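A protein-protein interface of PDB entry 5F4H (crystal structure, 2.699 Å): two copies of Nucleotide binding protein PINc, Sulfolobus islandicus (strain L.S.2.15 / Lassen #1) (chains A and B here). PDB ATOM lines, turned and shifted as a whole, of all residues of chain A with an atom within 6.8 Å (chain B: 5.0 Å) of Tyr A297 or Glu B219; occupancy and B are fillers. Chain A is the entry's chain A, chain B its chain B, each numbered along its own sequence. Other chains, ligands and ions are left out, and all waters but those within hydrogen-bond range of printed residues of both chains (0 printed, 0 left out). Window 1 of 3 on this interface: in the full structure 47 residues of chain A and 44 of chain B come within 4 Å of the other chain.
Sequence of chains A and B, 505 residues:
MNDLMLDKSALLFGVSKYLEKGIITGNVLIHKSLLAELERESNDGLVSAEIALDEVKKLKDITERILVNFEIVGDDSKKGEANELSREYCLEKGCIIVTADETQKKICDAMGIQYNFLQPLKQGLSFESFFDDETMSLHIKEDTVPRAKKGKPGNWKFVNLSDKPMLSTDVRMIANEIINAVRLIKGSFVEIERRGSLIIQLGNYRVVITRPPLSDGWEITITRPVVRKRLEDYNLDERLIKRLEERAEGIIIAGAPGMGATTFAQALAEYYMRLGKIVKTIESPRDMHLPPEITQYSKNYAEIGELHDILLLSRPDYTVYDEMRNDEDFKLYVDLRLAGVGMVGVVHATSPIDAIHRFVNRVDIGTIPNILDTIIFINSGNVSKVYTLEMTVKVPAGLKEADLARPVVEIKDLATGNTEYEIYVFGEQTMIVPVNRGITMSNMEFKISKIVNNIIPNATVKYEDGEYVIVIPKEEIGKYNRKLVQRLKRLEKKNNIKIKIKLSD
OE2 of Glu B219 lies within salt-bridge range of NZ of Lys A280 (2.8 Å). The guanidinium group (NH1) of Arg A286 sits at hydrogen-bond distance from the backbone carbonyl oxygen (O) of Leu B214 (3.4 Å). OG1 of Thr A295 lies within hydrogen-bond range of OE2 of Glu B219 (2.6 Å). OH of Tyr A297 lies within hydrogen-bond range of OE1 of Glu B219 (2.9 Å). O of Leu B214 is in hydrogen-bond range of N of Ser A298 (2.7 Å).
NE2 of Gln A296 is in hydrogen-bond range of OE2 of Glu A283, at 2.8 Å. The guanidinium group of Arg A286 is in hydrogen-bond range of the backbone carbonyl oxygen of Gln A296, at 3.0 Å. OD1 of Asn A300 sits at hydrogen-bond distance from OG of Ser A298 (2.8 Å). The backbone NH (N) of Val B208 sits at hydrogen-bond distance from the backbone carbonyl oxygen (O) of Thr B221, at 2.9 Å. OG of Ser B215 sits at hydrogen-bond distance from OG1 of Thr B210 (3.2 Å). OG of Ser B215 sits at hydrogen-bond distance from O of Gly B217 (2.6 Å).
Among the printed residues, pairs that only touch across the chains: Arg A286 with Ser B215, Pro A292 with Lys B141, Thr A295 with Lys B141, Gln A296 with Leu B214, Gln A296 with Ser B215, Tyr A297 with Leu B214, Tyr A297 with Ser B215, Ala A302 with Leu B214, Ile A310 with Val B208, Ile A310 with Thr B210 and Ser A314 with Thr B221.
Tyr A297 touches just these residues of chain B: Leu B214, Ser B215 and Glu B219. Of the printed residues of chain B, Ser A314 touches Thr B221. Val B171 touches none of the printed residues of chain A. Of the printed residues of chain A, Thr B210 touches Ile A310. Glu B219 touches three residues of chain A. Of the printed residues of chain A, Thr B221 touches Ser A314 (3.4 Å). The nearest residue of chain B that does not touch Tyr A297 is Thr B210 (4.02 Å). The nearest residue of chain A that does not touch Glu B219 is Ile A310 (5.8 Å).
Printed residues of chain A that touch a printed residue of chain B: Lys A280, Arg A286, Pro A292, Thr A295, Gln A296, Tyr A297, Ser A298, Ala A302, Ile A310 and Ser A314. Hydrophobic or aromatic side chains of chain A within 4 Å of the printed part of chain B: Tyr A297, Ala A302 and Ile A310. Among the printed residues, 16 pairs touch across the chains. Among the printed residues, Asp or Glu carboxylates within 4 Å of a Lys or Arg side-chain nitrogen of the other chain: Lys A280 with Glu B219.
No position is printed for both chains. Of the 16 pairs that touch across the chains among the printed residues, none has its exchanged pair printed and touching as well.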
ATOM      1  N   ILE A 278       4.981  13.224 -24.711  1.00  0.00           N
ATOM      2  CA  ILE A 278       3.813  14.121 -24.907  1.00  0.00           C
ATOM      3  C   ILE A 278       2.618  13.464 -24.256  1.00  0.00           C
ATOM      4  O   ILE A 278       2.284  12.310 -24.578  1.00  0.00           O
ATOM      5  CB  ILE A 278       3.507  14.402 -26.371  1.00  0.00           C
ATOM      6  CG1 ILE A 278       4.518  15.423 -26.892  1.00  0.00           C
ATOM      7  CG2 ILE A 278       2.150  15.014 -26.558  1.00  0.00           C
ATOM      8  CD1 ILE A 278       4.999  15.024 -28.267  1.00  0.00           C
ATOM      9  N   VAL A 279       2.045  14.154 -23.278  1.00  0.00           N
ATOM     10  CA  VAL A 279       0.972  13.573 -22.505  1.00  0.00           C
ATOM     11  C   VAL A 279      -0.231  14.440 -22.578  1.00  0.00           C
ATOM     12  O   VAL A 279      -0.127  15.664 -22.575  1.00  0.00           O
ATOM     13  CB  VAL A 279       1.337  13.397 -21.030  1.00  0.00           C
ATOM     14  CG1 VAL A 279       0.258  12.619 -20.290  1.00  0.00           C
ATOM     15  CG2 VAL A 279       2.638  12.645 -20.924  1.00  0.00           C
ATOM     16  N   LYS A 280      -1.379  13.786 -22.611  1.00  0.00           N
ATOM     17  CA  LYS A 280      -2.670  14.449 -22.635  1.00  0.00           C
ATOM     18  C   LYS A 280      -3.593  13.692 -21.745  1.00  0.00           C
ATOM     19  O   LYS A 280      -3.317  12.578 -21.419  1.00  0.00           O
ATOM     20  CB  LYS A 280      -3.245  14.501 -24.070  1.00  0.00           C
ATOM     21  CG  LYS A 280      -2.560  15.589 -24.852  1.00  0.00           C
ATOM     22  CD  LYS A 280      -2.432  15.298 -26.307  1.00  0.00           C
ATOM     23  CE  LYS A 280      -2.732  16.556 -27.135  1.00  0.00           C
ATOM     24  NZ  LYS A 280      -1.640  17.514 -27.288  1.00  0.00           N
ATOM     25  N   THR A 281      -4.665  14.338 -21.339  1.00  0.00           N
ATOM     26  CA  THR A 281      -5.643  13.684 -20.498  1.00  0.00           C
ATOM     27  C   THR A 281      -7.043  13.936 -20.996  1.00  0.00           C
ATOM     28  O   THR A 281      -7.292  14.950 -21.663  1.00  0.00           O
ATOM     29  CB  THR A 281      -5.531  14.123 -19.009  1.00  0.00           C
ATOM     30  OG1 THR A 281      -6.158  15.406 -18.796  1.00  0.00           O
ATOM     31  CG2 THR A 281      -4.065  14.179 -18.572  1.00  0.00           C
ATOM     32  N   ILE A 282      -7.915  13.005 -20.664  1.00  0.00           N
ATOM     33  CA  ILE A 282      -9.332  13.151 -20.903  1.00  0.00           C
ATOM     34  C   ILE A 282     -10.013  13.006 -19.578  1.00  0.00           C
ATOM     35  O   ILE A 282      -9.860  11.965 -18.923  1.00  0.00           O
ATOM     36  CB  ILE A 282      -9.858  12.016 -21.788  1.00  0.00           C
ATOM     37  CG1 ILE A 282      -9.195  12.090 -23.141  1.00  0.00           C
ATOM     38  CG2 ILE A 282     -11.342  12.136 -21.948  1.00  0.00           C
ATOM     39  CD1 ILE A 282      -9.583  10.952 -24.069  1.00  0.00           C
ATOM     40  N   GLU A 283     -10.780  13.992 -19.176  1.00  0.00           N
ATOM     41  CA  GLU A 283     -11.401  13.954 -17.851  1.00  0.00           C
ATOM     42  C   GLU A 283     -12.810  14.493 -17.880  1.00  0.00           C
ATOM     43  O   GLU A 283     -13.167  15.183 -18.821  1.00  0.00           O
ATOM     44  CB  GLU A 283     -10.574  14.752 -16.821  1.00  0.00           C
ATOM     45  CG  GLU A 283      -9.072  14.817 -17.080  1.00  0.00           C
ATOM     46  CD  GLU A 283      -8.275  15.636 -16.071  1.00  0.00           C
ATOM     47  OE1 GLU A 283      -8.639  15.730 -14.893  1.00  0.00           O
ATOM     48  OE2 GLU A 283      -7.253  16.196 -16.441  1.00  0.00           O
ATOM     49  N   SER A 284     -13.593  14.167 -16.865  1.00  0.00           N
ATOM     50  CA  SER A 284     -14.959  14.621 -16.828  1.00  0.00           C
ATOM     51  C   SER A 284     -15.549  14.702 -15.389  1.00  0.00           C
ATOM     52  O   SER A 284     -15.938  13.681 -14.825  1.00  0.00           O
ATOM     53  CB  SER A 284     -15.865  13.729 -17.772  1.00  0.00           C
ATOM     54  OG  SER A 284     -17.184  13.492 -17.272  1.00  0.00           O
ATOM     55  N   PRO A 285     -15.606  15.898 -14.813  1.00  0.00           N
ATOM     56  CA  PRO A 285     -14.988  17.084 -15.417  1.00  0.00           C
ATOM     57  C   PRO A 285     -13.499  17.205 -15.130  1.00  0.00           C
ATOM     58  O   PRO A 285     -12.932  16.410 -14.420  1.00  0.00           O
ATOM     59  CB  PRO A 285     -15.703  18.194 -14.722  1.00  0.00           C
ATOM     60  CG  PRO A 285     -15.759  17.693 -13.309  1.00  0.00           C
ATOM     61  CD  PRO A 285     -16.037  16.206 -13.439  1.00  0.00           C
ATOM     62  N   ARG A 286     -12.863  18.181 -15.715  1.00  0.00           N
ATOM     63  CA  ARG A 286     -11.417  18.329 -15.566  1.00  0.00           C
ATOM     64  C   ARG A 286     -11.078  18.773 -14.164  1.00  0.00           C
ATOM     65  O   ARG A 286     -11.574  19.791 -13.746  1.00  0.00           O
ATOM     66  CB  ARG A 286     -10.902  19.361 -16.586  1.00  0.00           C
ATOM     67  CG  ARG A 286      -9.548  20.018 -16.279  1.00  0.00           C
ATOM     68  CD  ARG A 286      -8.982  20.856 -17.418  1.00  0.00           C
ATOM     69  NE  ARG A 286      -9.827  21.974 -17.737  1.00  0.00           N
ATOM     70  CZ  ARG A 286     -10.496  22.046 -18.912  1.00  0.00           C
ATOM     71  NH1 ARG A 286     -10.313  21.109 -19.875  1.00  0.00           N
ATOM     72  NH2 ARG A 286     -11.355  23.044 -19.155  1.00  0.00           N
ATOM     73  N   PRO A 292       1.060  23.030 -17.372  1.00  0.00           N
ATOM     74  CA  PRO A 292       0.510  23.302 -18.706  1.00  0.00           C
ATOM     75  C   PRO A 292       1.160  22.515 -19.847  1.00  0.00           C
ATOM     76  O   PRO A 292       0.595  22.395 -20.928  1.00  0.00           O
ATOM     77  CB  PRO A 292       0.818  24.769 -18.897  1.00  0.00           C
ATOM     78  CG  PRO A 292       0.978  25.314 -17.520  1.00  0.00           C
ATOM     79  CD  PRO A 292       1.705  24.225 -16.823  1.00  0.00           C
ATOM     80  N   GLU A 293       2.315  21.935 -19.580  1.00  0.00           N
ATOM     81  CA  GLU A 293       3.039  21.091 -20.523  1.00  0.00           C
ATOM     82  C   GLU A 293       2.151  19.863 -20.874  1.00  0.00           C
ATOM     83  O   GLU A 293       2.184  19.340 -21.984  1.00  0.00           O
ATOM     84  CB  GLU A 293       4.401  20.647 -19.919  1.00  0.00           C
ATOM     85  CG  GLU A 293       5.109  21.551 -18.869  1.00  0.00           C
ATOM     86  CD  GLU A 293       5.389  22.928 -19.331  1.00  0.00           C
ATOM     87  OE1 GLU A 293       5.676  23.145 -20.526  1.00  0.00           O
ATOM     88  OE2 GLU A 293       5.294  23.800 -18.472  1.00  0.00           O
ATOM     89  N   ILE A 294       1.258  19.479 -19.971  1.00  0.00           N
ATOM     90  CA  ILE A 294       0.275  18.431 -20.257  1.00  0.00           C
ATOM     91  C   ILE A 294      -1.108  19.011 -20.576  1.00  0.00           C
ATOM     92  O   ILE A 294      -1.702  19.692 -19.763  1.00  0.00           O
ATOM     93  CB  ILE A 294       0.117  17.535 -19.057  1.00  0.00           C
ATOM     94  CG1 ILE A 294       1.411  16.821 -18.804  1.00  0.00           C
ATOM     95  CG2 ILE A 294      -1.011  16.537 -19.269  1.00  0.00           C
ATOM     96  CD1 ILE A 294       1.385  16.006 -17.538  1.00  0.00           C
ATOM     97  N   THR A 295      -1.671  18.645 -21.717  1.00  0.00           N
ATOM     98  CA  THR A 295      -2.960  19.186 -22.119  1.00  0.00           C
ATOM     99  C   THR A 295      -4.090  18.393 -21.545  1.00  0.00           C
ATOM    100  O   THR A 295      -4.122  17.174 -21.669  1.00  0.00           O
ATOM    101  CB  THR A 295      -3.089  19.219 -23.656  1.00  0.00           C
ATOM    102  OG1 THR A 295      -2.152  20.154 -24.209  1.00  0.00           O
ATOM    103  CG2 THR A 295      -4.439  19.681 -24.114  1.00  0.00           C
ATOM    104  N   GLN A 296      -5.057  19.077 -20.969  1.00  0.00           N
ATOM    105  CA  GLN A 296      -6.184  18.380 -20.342  1.00  0.00           C
ATOM    106  C   GLN A 296      -7.518  18.659 -21.039  1.00  0.00           C
ATOM    107  O   GLN A 296      -7.947  19.815 -21.115  1.00  0.00           O
ATOM    108  CB  GLN A 296      -6.293  18.751 -18.884  1.00  0.00           C
ATOM    109  CG  GLN A 296      -4.959  18.660 -18.153  1.00  0.00           C
ATOM    110  CD  GLN A 296      -4.969  19.157 -16.696  1.00  0.00           C
ATOM    111  OE1 GLN A 296      -4.280  20.116 -16.334  1.00  0.00           O
ATOM    112  NE2 GLN A 296      -5.713  18.446 -15.858  1.00  0.00           N
ATOM    113  N   TYR A 297      -8.120  17.611 -21.613  1.00  0.00           N
ATOM    114  CA  TYR A 297      -9.345  17.775 -22.399  1.00  0.00           C
ATOM    115  C   TYR A 297     -10.515  17.477 -21.508  1.00  0.00           C
ATOM    116  O   TYR A 297     -10.482  16.563 -20.707  1.00  0.00           O
ATOM    117  CB  TYR A 297      -9.374  16.878 -23.619  1.00  0.00           C
ATOM    118  CG  TYR A 297      -8.315  17.190 -24.663  1.00  0.00           C
ATOM    119  CD1 TYR A 297      -8.257  18.389 -25.278  1.00  0.00           C
ATOM    120  CD2 TYR A 297      -7.374  16.276 -25.016  1.00  0.00           C
ATOM    121  CE1 TYR A 297      -7.275  18.699 -26.211  1.00  0.00           C
ATOM    122  CE2 TYR A 297      -6.379  16.566 -25.980  1.00  0.00           C
ATOM    123  CZ  TYR A 297      -6.337  17.797 -26.565  1.00  0.00           C
ATOM    124  OH  TYR A 297      -5.400  18.135 -27.486  1.00  0.00           O
ATOM    125  N   SER A 298     -11.532  18.310 -21.567  1.00  0.00           N
ATOM    126  CA  SER A 298     -12.756  18.056 -20.827  1.00  0.00           C
ATOM    127  C   SER A 298     -13.776  17.366 -21.712  1.00  0.00           C
ATOM    128  O   SER A 298     -14.384  17.976 -22.552  1.00  0.00           O
ATOM    129  CB  SER A 298     -13.343  19.395 -20.417  1.00  0.00           C
ATOM    130  OG  SER A 298     -14.190  19.318 -19.303  1.00  0.00           O
ATOM    131  N   LYS A 299     -13.948  16.082 -21.497  1.00  0.00           N
ATOM    132  CA  LYS A 299     -14.799  15.270 -22.296  1.00  0.00           C
ATOM    133  C   LYS A 299     -16.222  15.789 -22.421  1.00  0.00           C
ATOM    134  O   LYS A 299     -16.818  15.673 -23.462  1.00  0.00           O
ATOM    135  CB  LYS A 299     -14.811  13.894 -21.673  1.00  0.00           C
ATOM    136  CG  LYS A 299     -15.404  12.824 -22.492  1.00  0.00           C
ATOM    137  CD  LYS A 299     -15.509  11.537 -21.675  1.00  0.00           C
ATOM    138  CE  LYS A 299     -16.887  11.430 -21.016  1.00  0.00           C
ATOM    139  NZ  LYS A 299     -17.034  10.118 -20.323  1.00  0.00           N
ATOM    140  N   ASN A 300     -16.768  16.361 -21.362  1.00  0.00           N
ATOM    141  CA  ASN A 300     -18.138  16.814 -21.369  1.00  0.00           C
ATOM    142  C   ASN A 300     -18.375  17.863 -22.407  1.00  0.00           C
ATOM    143  O   ASN A 300     -19.486  18.022 -22.886  1.00  0.00           O
ATOM    144  CB  ASN A 300     -18.616  17.373 -20.020  1.00  0.00           C
ATOM    145  CG  ASN A 300     -17.521  17.390 -18.926  1.00  0.00           C
ATOM    146  OD1 ASN A 300     -16.753  18.341 -18.733  1.00  0.00           O
ATOM    147  ND2 ASN A 300     -17.483  16.295 -18.171  1.00  0.00           N
ATOM    148  N   ALA A 302     -16.899  18.049 -25.300  1.00  0.00           N
ATOM    149  CA  ALA A 302     -16.482  17.591 -26.595  1.00  0.00           C
ATOM    150  C   ALA A 302     -17.645  16.983 -27.345  1.00  0.00           C
ATOM    151  O   ALA A 302     -18.478  16.292 -26.777  1.00  0.00           O
ATOM    152  CB  ALA A 302     -15.407  16.607 -26.440  1.00  0.00           C
ATOM    153  N   LEU A 307     -12.820  14.263 -29.777  1.00  0.00           N
ATOM    154  CA  LEU A 307     -11.568  13.845 -29.168  1.00  0.00           C
ATOM    155  C   LEU A 307     -10.812  12.798 -29.979  1.00  0.00           C
ATOM    156  O   LEU A 307      -9.617  12.795 -30.017  1.00  0.00           O
ATOM    157  CB  LEU A 307     -11.822  13.304 -27.743  1.00  0.00           C
ATOM    158  CG  LEU A 307     -12.149  14.387 -26.738  1.00  0.00           C
ATOM    159  CD1 LEU A 307     -12.322  13.785 -25.371  1.00  0.00           C
ATOM    160  CD2 LEU A 307     -11.059  15.421 -26.677  1.00  0.00           C
ATOM    161  N   ILE A 310      -9.069  14.452 -32.809  1.00  0.00           N
ATOM    162  CA  ILE A 310      -7.988  15.291 -32.349  1.00  0.00           C
ATOM    163  C   ILE A 310      -6.768  14.457 -31.912  1.00  0.00           C
ATOM    164  O   ILE A 310      -5.640  14.760 -32.254  1.00  0.00           O
ATOM    165  CB  ILE A 310      -8.452  16.164 -31.178  1.00  0.00           C
ATOM    166  CG1 ILE A 310      -9.433  17.191 -31.727  1.00  0.00           C
ATOM    167  CG2 ILE A 310      -7.277  16.884 -30.518  1.00  0.00           C
ATOM    168  CD1 ILE A 310     -10.028  18.091 -30.676  1.00  0.00           C
ATOM    169  N   LEU A 311      -7.031  13.447 -31.099  1.00  0.00           N
ATOM    170  CA  LEU A 311      -5.999  12.625 -30.567  1.00  0.00           C
ATOM    171  C   LEU A 311      -5.302  11.839 -31.652  1.00  0.00           C
ATOM    172  O   LEU A 311      -4.133  11.553 -31.521  1.00  0.00           O
ATOM    173  CB  LEU A 311      -6.560  11.701 -29.516  1.00  0.00           C
ATOM    174  CG  LEU A 311      -6.898  12.416 -28.229  1.00  0.00           C
ATOM    175  CD1 LEU A 311      -7.654  11.521 -27.280  1.00  0.00           C
ATOM    176  CD2 LEU A 311      -5.651  12.908 -27.509  1.00  0.00           C
ATOM    177  N   SER A 314      -3.099  14.389 -33.751  1.00  0.00           N
ATOM    178  CA  SER A 314      -1.905  14.776 -33.038  1.00  0.00           C
ATOM    179  C   SER A 314      -1.497  13.694 -32.050  1.00  0.00           C
ATOM    180  O   SER A 314      -1.733  13.810 -30.849  1.00  0.00           O
ATOM    181  CB  SER A 314      -2.149  16.098 -32.390  1.00  0.00           C
ATOM    182  OG  SER A 314      -1.290  16.169 -31.309  1.00  0.00           O
ATOM    183  N   THR A 319      -2.074   9.087 -23.266  1.00  0.00           N
ATOM    184  CA  THR A 319      -3.278   9.765 -22.964  1.00  0.00           C
ATOM    185  C   THR A 319      -3.810   9.145 -21.710  1.00  0.00           C
ATOM    186  O   THR A 319      -3.983   7.926 -21.624  1.00  0.00           O
ATOM    187  CB  THR A 319      -4.303   9.585 -24.083  1.00  0.00           C
ATOM    188  OG1 THR A 319      -3.756  10.096 -25.296  1.00  0.00           O
ATOM    189  CG2 THR A 319      -5.605  10.352 -23.782  1.00  0.00           C
ATOM    190  N   ILE B 140       2.587  23.716 -29.727  1.00  0.00           N
ATOM    191  CA  ILE B 140       2.539  25.038 -29.170  1.00  0.00           C
ATOM    192  C   ILE B 140       1.363  25.153 -28.250  1.00  0.00           C
ATOM    193  O   ILE B 140       0.267  24.852 -28.642  1.00  0.00           O
ATOM    194  CB  ILE B 140       2.352  26.071 -30.273  1.00  0.00           C
ATOM    195  CG1 ILE B 140       3.600  26.036 -31.179  1.00  0.00           C
ATOM    196  CG2 ILE B 140       2.118  27.454 -29.688  1.00  0.00           C
ATOM    197  CD1 ILE B 140       3.463  26.896 -32.407  1.00  0.00           C
ATOM    198  N   LYS B 141       1.608  25.634 -27.048  1.00  0.00           N
ATOM    199  CA  LYS B 141       0.574  25.805 -26.055  1.00  0.00           C
ATOM    200  C   LYS B 141       0.891  27.014 -25.187  1.00  0.00           C
ATOM    201  O   LYS B 141       2.028  27.373 -24.993  1.00  0.00           O
ATOM    202  CB  LYS B 141       0.505  24.585 -25.169  1.00  0.00           C
ATOM    203  CG  LYS B 141      -0.730  24.545 -24.358  1.00  0.00           C
ATOM    204  CD  LYS B 141      -0.877  23.251 -23.607  1.00  0.00           C
ATOM    205  CE  LYS B 141      -2.224  22.914 -23.005  1.00  0.00           C
ATOM    206  NZ  LYS B 141      -2.499  23.807 -21.875  1.00  0.00           N
ATOM    207  N   VAL B 171       0.109  32.775 -28.991  1.00  0.00           N
ATOM    208  CA  VAL B 171      -0.518  31.574 -29.546  1.00  0.00           C
ATOM    209  C   VAL B 171      -1.709  31.935 -30.420  1.00  0.00           C
ATOM    210  O   VAL B 171      -1.857  31.419 -31.504  1.00  0.00           O
ATOM    211  CB  VAL B 171      -0.999  30.639 -28.460  1.00  0.00           C
ATOM    212  CG1 VAL B 171      -1.682  29.432 -29.059  1.00  0.00           C
ATOM    213  CG2 VAL B 171       0.176  30.169 -27.633  1.00  0.00           C
ATOM    214  N   VAL B 208      -4.207  21.337 -35.858  1.00  0.00           N
ATOM    215  CA  VAL B 208      -5.280  21.159 -34.899  1.00  0.00           C
ATOM    216  C   VAL B 208      -5.171  22.221 -33.835  1.00  0.00           C
ATOM    217  O   VAL B 208      -4.117  22.315 -33.182  1.00  0.00           O
ATOM    218  CB  VAL B 208      -5.155  19.808 -34.205  1.00  0.00           C
ATOM    219  CG1 VAL B 208      -6.306  19.598 -33.231  1.00  0.00           C
ATOM    220  CG2 VAL B 208      -5.139  18.711 -35.248  1.00  0.00           C
ATOM    221  N   ILE B 209      -6.258  22.954 -33.632  1.00  0.00           N
ATOM    222  CA  ILE B 209      -6.272  23.973 -32.672  1.00  0.00           C
ATOM    223  C   ILE B 209      -7.324  23.709 -31.654  1.00  0.00           C
ATOM    224  O   ILE B 209      -8.461  23.422 -32.026  1.00  0.00           O
ATOM    225  CB  ILE B 209      -6.545  25.291 -33.317  1.00  0.00           C
ATOM    226  CG1 ILE B 209      -5.478  25.569 -34.374  1.00  0.00           C
ATOM    227  CG2 ILE B 209      -6.531  26.407 -32.271  1.00  0.00           C
ATOM    228  CD1 ILE B 209      -5.618  26.902 -35.101  1.00  0.00           C
ATOM    229  N   THR B 210      -6.971  23.826 -30.368  1.00  0.00           N
ATOM    230  CA  THR B 210      -7.956  23.642 -29.290  1.00  0.00           C
ATOM    231  C   THR B 210      -7.928  24.781 -28.343  1.00  0.00           C
ATOM    232  O   THR B 210      -6.904  25.426 -28.227  1.00  0.00           O
ATOM    233  CB  THR B 210      -7.779  22.355 -28.467  1.00  0.00           C
ATOM    234  OG1 THR B 210      -6.480  22.272 -27.879  1.00  0.00           O
ATOM    235  CG2 THR B 210      -7.992  21.186 -29.367  1.00  0.00           C
ATOM    236  N   LEU B 214     -12.656  23.333 -23.896  1.00  0.00           N
ATOM    237  CA  LEU B 214     -12.347  21.954 -24.285  1.00  0.00           C
ATOM    238  C   LEU B 214     -10.971  21.508 -23.729  1.00  0.00           C
ATOM    239  O   LEU B 214     -10.846  20.436 -23.164  1.00  0.00           O
ATOM    240  CB  LEU B 214     -12.346  21.800 -25.792  1.00  0.00           C
ATOM    241  CG  LEU B 214     -11.943  20.425 -26.258  1.00  0.00           C
ATOM    242  CD1 LEU B 214     -12.925  19.391 -25.796  1.00  0.00           C
ATOM    243  CD2 LEU B 214     -11.891  20.438 -27.760  1.00  0.00           C
ATOM    244  N   SER B 215     -10.003  22.397 -23.868  1.00  0.00           N
ATOM    245  CA  SER B 215      -8.672  22.167 -23.381  1.00  0.00           C
ATOM    246  C   SER B 215      -8.353  23.196 -22.304  1.00  0.00           C
ATOM    247  O   SER B 215      -8.939  24.244 -22.273  1.00  0.00           O
ATOM    248  CB  SER B 215      -7.690  22.211 -24.555  1.00  0.00           C
ATOM    249  OG  SER B 215      -7.548  23.491 -25.130  1.00  0.00           O
ATOM    250  N   GLY B 217      -5.787  25.087 -21.962  1.00  0.00           N
ATOM    251  CA  GLY B 217      -5.252  26.318 -22.552  1.00  0.00           C
ATOM    252  C   GLY B 217      -5.341  26.231 -24.046  1.00  0.00           C
ATOM    253  O   GLY B 217      -5.671  25.163 -24.591  1.00  0.00           O
ATOM    254  N   TRP B 218      -4.992  27.322 -24.716  1.00  0.00           N
ATOM    255  CA  TRP B 218      -4.869  27.327 -26.176  1.00  0.00           C
ATOM    256  C   TRP B 218      -3.706  26.453 -26.624  1.00  0.00           C
ATOM    257  O   TRP B 218      -2.614  26.585 -26.169  1.00  0.00           O
ATOM    258  CB  TRP B 218      -4.652  28.717 -26.728  1.00  0.00           C
ATOM    259  CG  TRP B 218      -5.844  29.495 -26.752  1.00  0.00           C
ATOM    260  CD1 TRP B 218      -6.433  30.127 -25.704  1.00  0.00           C
ATOM    261  CD2 TRP B 218      -6.634  29.774 -27.872  1.00  0.00           C
ATOM    262  NE1 TRP B 218      -7.551  30.787 -26.093  1.00  0.00           N
ATOM    263  CE2 TRP B 218      -7.702  30.574 -27.433  1.00  0.00           C
ATOM    264  CE3 TRP B 218      -6.561  29.418 -29.222  1.00  0.00           C
ATOM    265  CZ2 TRP B 218      -8.691  30.998 -28.275  1.00  0.00           C
ATOM    266  CZ3 TRP B 218      -7.547  29.864 -30.070  1.00  0.00           C
ATOM    267  CH2 TRP B 218      -8.607  30.640 -29.584  1.00  0.00           C
ATOM    268  N   GLU B 219      -3.989  25.551 -27.550  1.00  0.00           N
ATOM    269  CA  GLU B 219      -2.990  24.622 -28.075  1.00  0.00           C
ATOM    270  C   GLU B 219      -3.080  24.507 -29.592  1.00  0.00           C
ATOM    271  O   GLU B 219      -4.159  24.478 -30.142  1.00  0.00           O
ATOM    272  CB  GLU B 219      -3.207  23.272 -27.492  1.00  0.00           C
ATOM    273  CG  GLU B 219      -2.109  22.295 -27.800  1.00  0.00           C
ATOM    274  CD  GLU B 219      -2.439  20.879 -27.324  1.00  0.00           C
ATOM    275  OE1 GLU B 219      -3.611  20.371 -27.600  1.00  0.00           O
ATOM    276  OE2 GLU B 219      -1.510  20.264 -26.698  1.00  0.00           O
ATOM    277  N   ILE B 220      -1.928  24.500 -30.235  1.00  0.00           N
ATOM    278  CA  ILE B 220      -1.836  24.374 -31.657  1.00  0.00           C
ATOM    279  C   ILE B 220      -0.842  23.321 -31.929  1.00  0.00           C
ATOM    280  O   ILE B 220       0.269  23.346 -31.416  1.00  0.00           O
ATOM    281  CB  ILE B 220      -1.296  25.614 -32.325  1.00  0.00           C
ATOM    282  CG1 ILE B 220      -2.161  26.804 -31.935  1.00  0.00           C
ATOM    283  CG2 ILE B 220      -1.354  25.435 -33.822  1.00  0.00           C
ATOM    284  CD1 ILE B 220      -1.762  28.097 -32.626  1.00  0.00           C
ATOM    285  N   THR B 221      -1.252  22.352 -32.720  1.00  0.00           N
ATOM    286  CA  THR B 221      -0.371  21.262 -33.113  1.00  0.00           C
ATOM    287  C   THR B 221      -0.344  21.229 -34.605  1.00  0.00           C
ATOM    288  O   THR B 221      -1.382  21.201 -35.244  1.00  0.00           O
ATOM    289  CB  THR B 221      -0.959  19.942 -32.680  1.00  0.00           C
ATOM    290  OG1 THR B 221      -1.420  20.033 -31.333  1.00  0.00           O
ATOM    291  CG2 THR B 221       0.052  18.900 -32.809  1.00  0.00           C
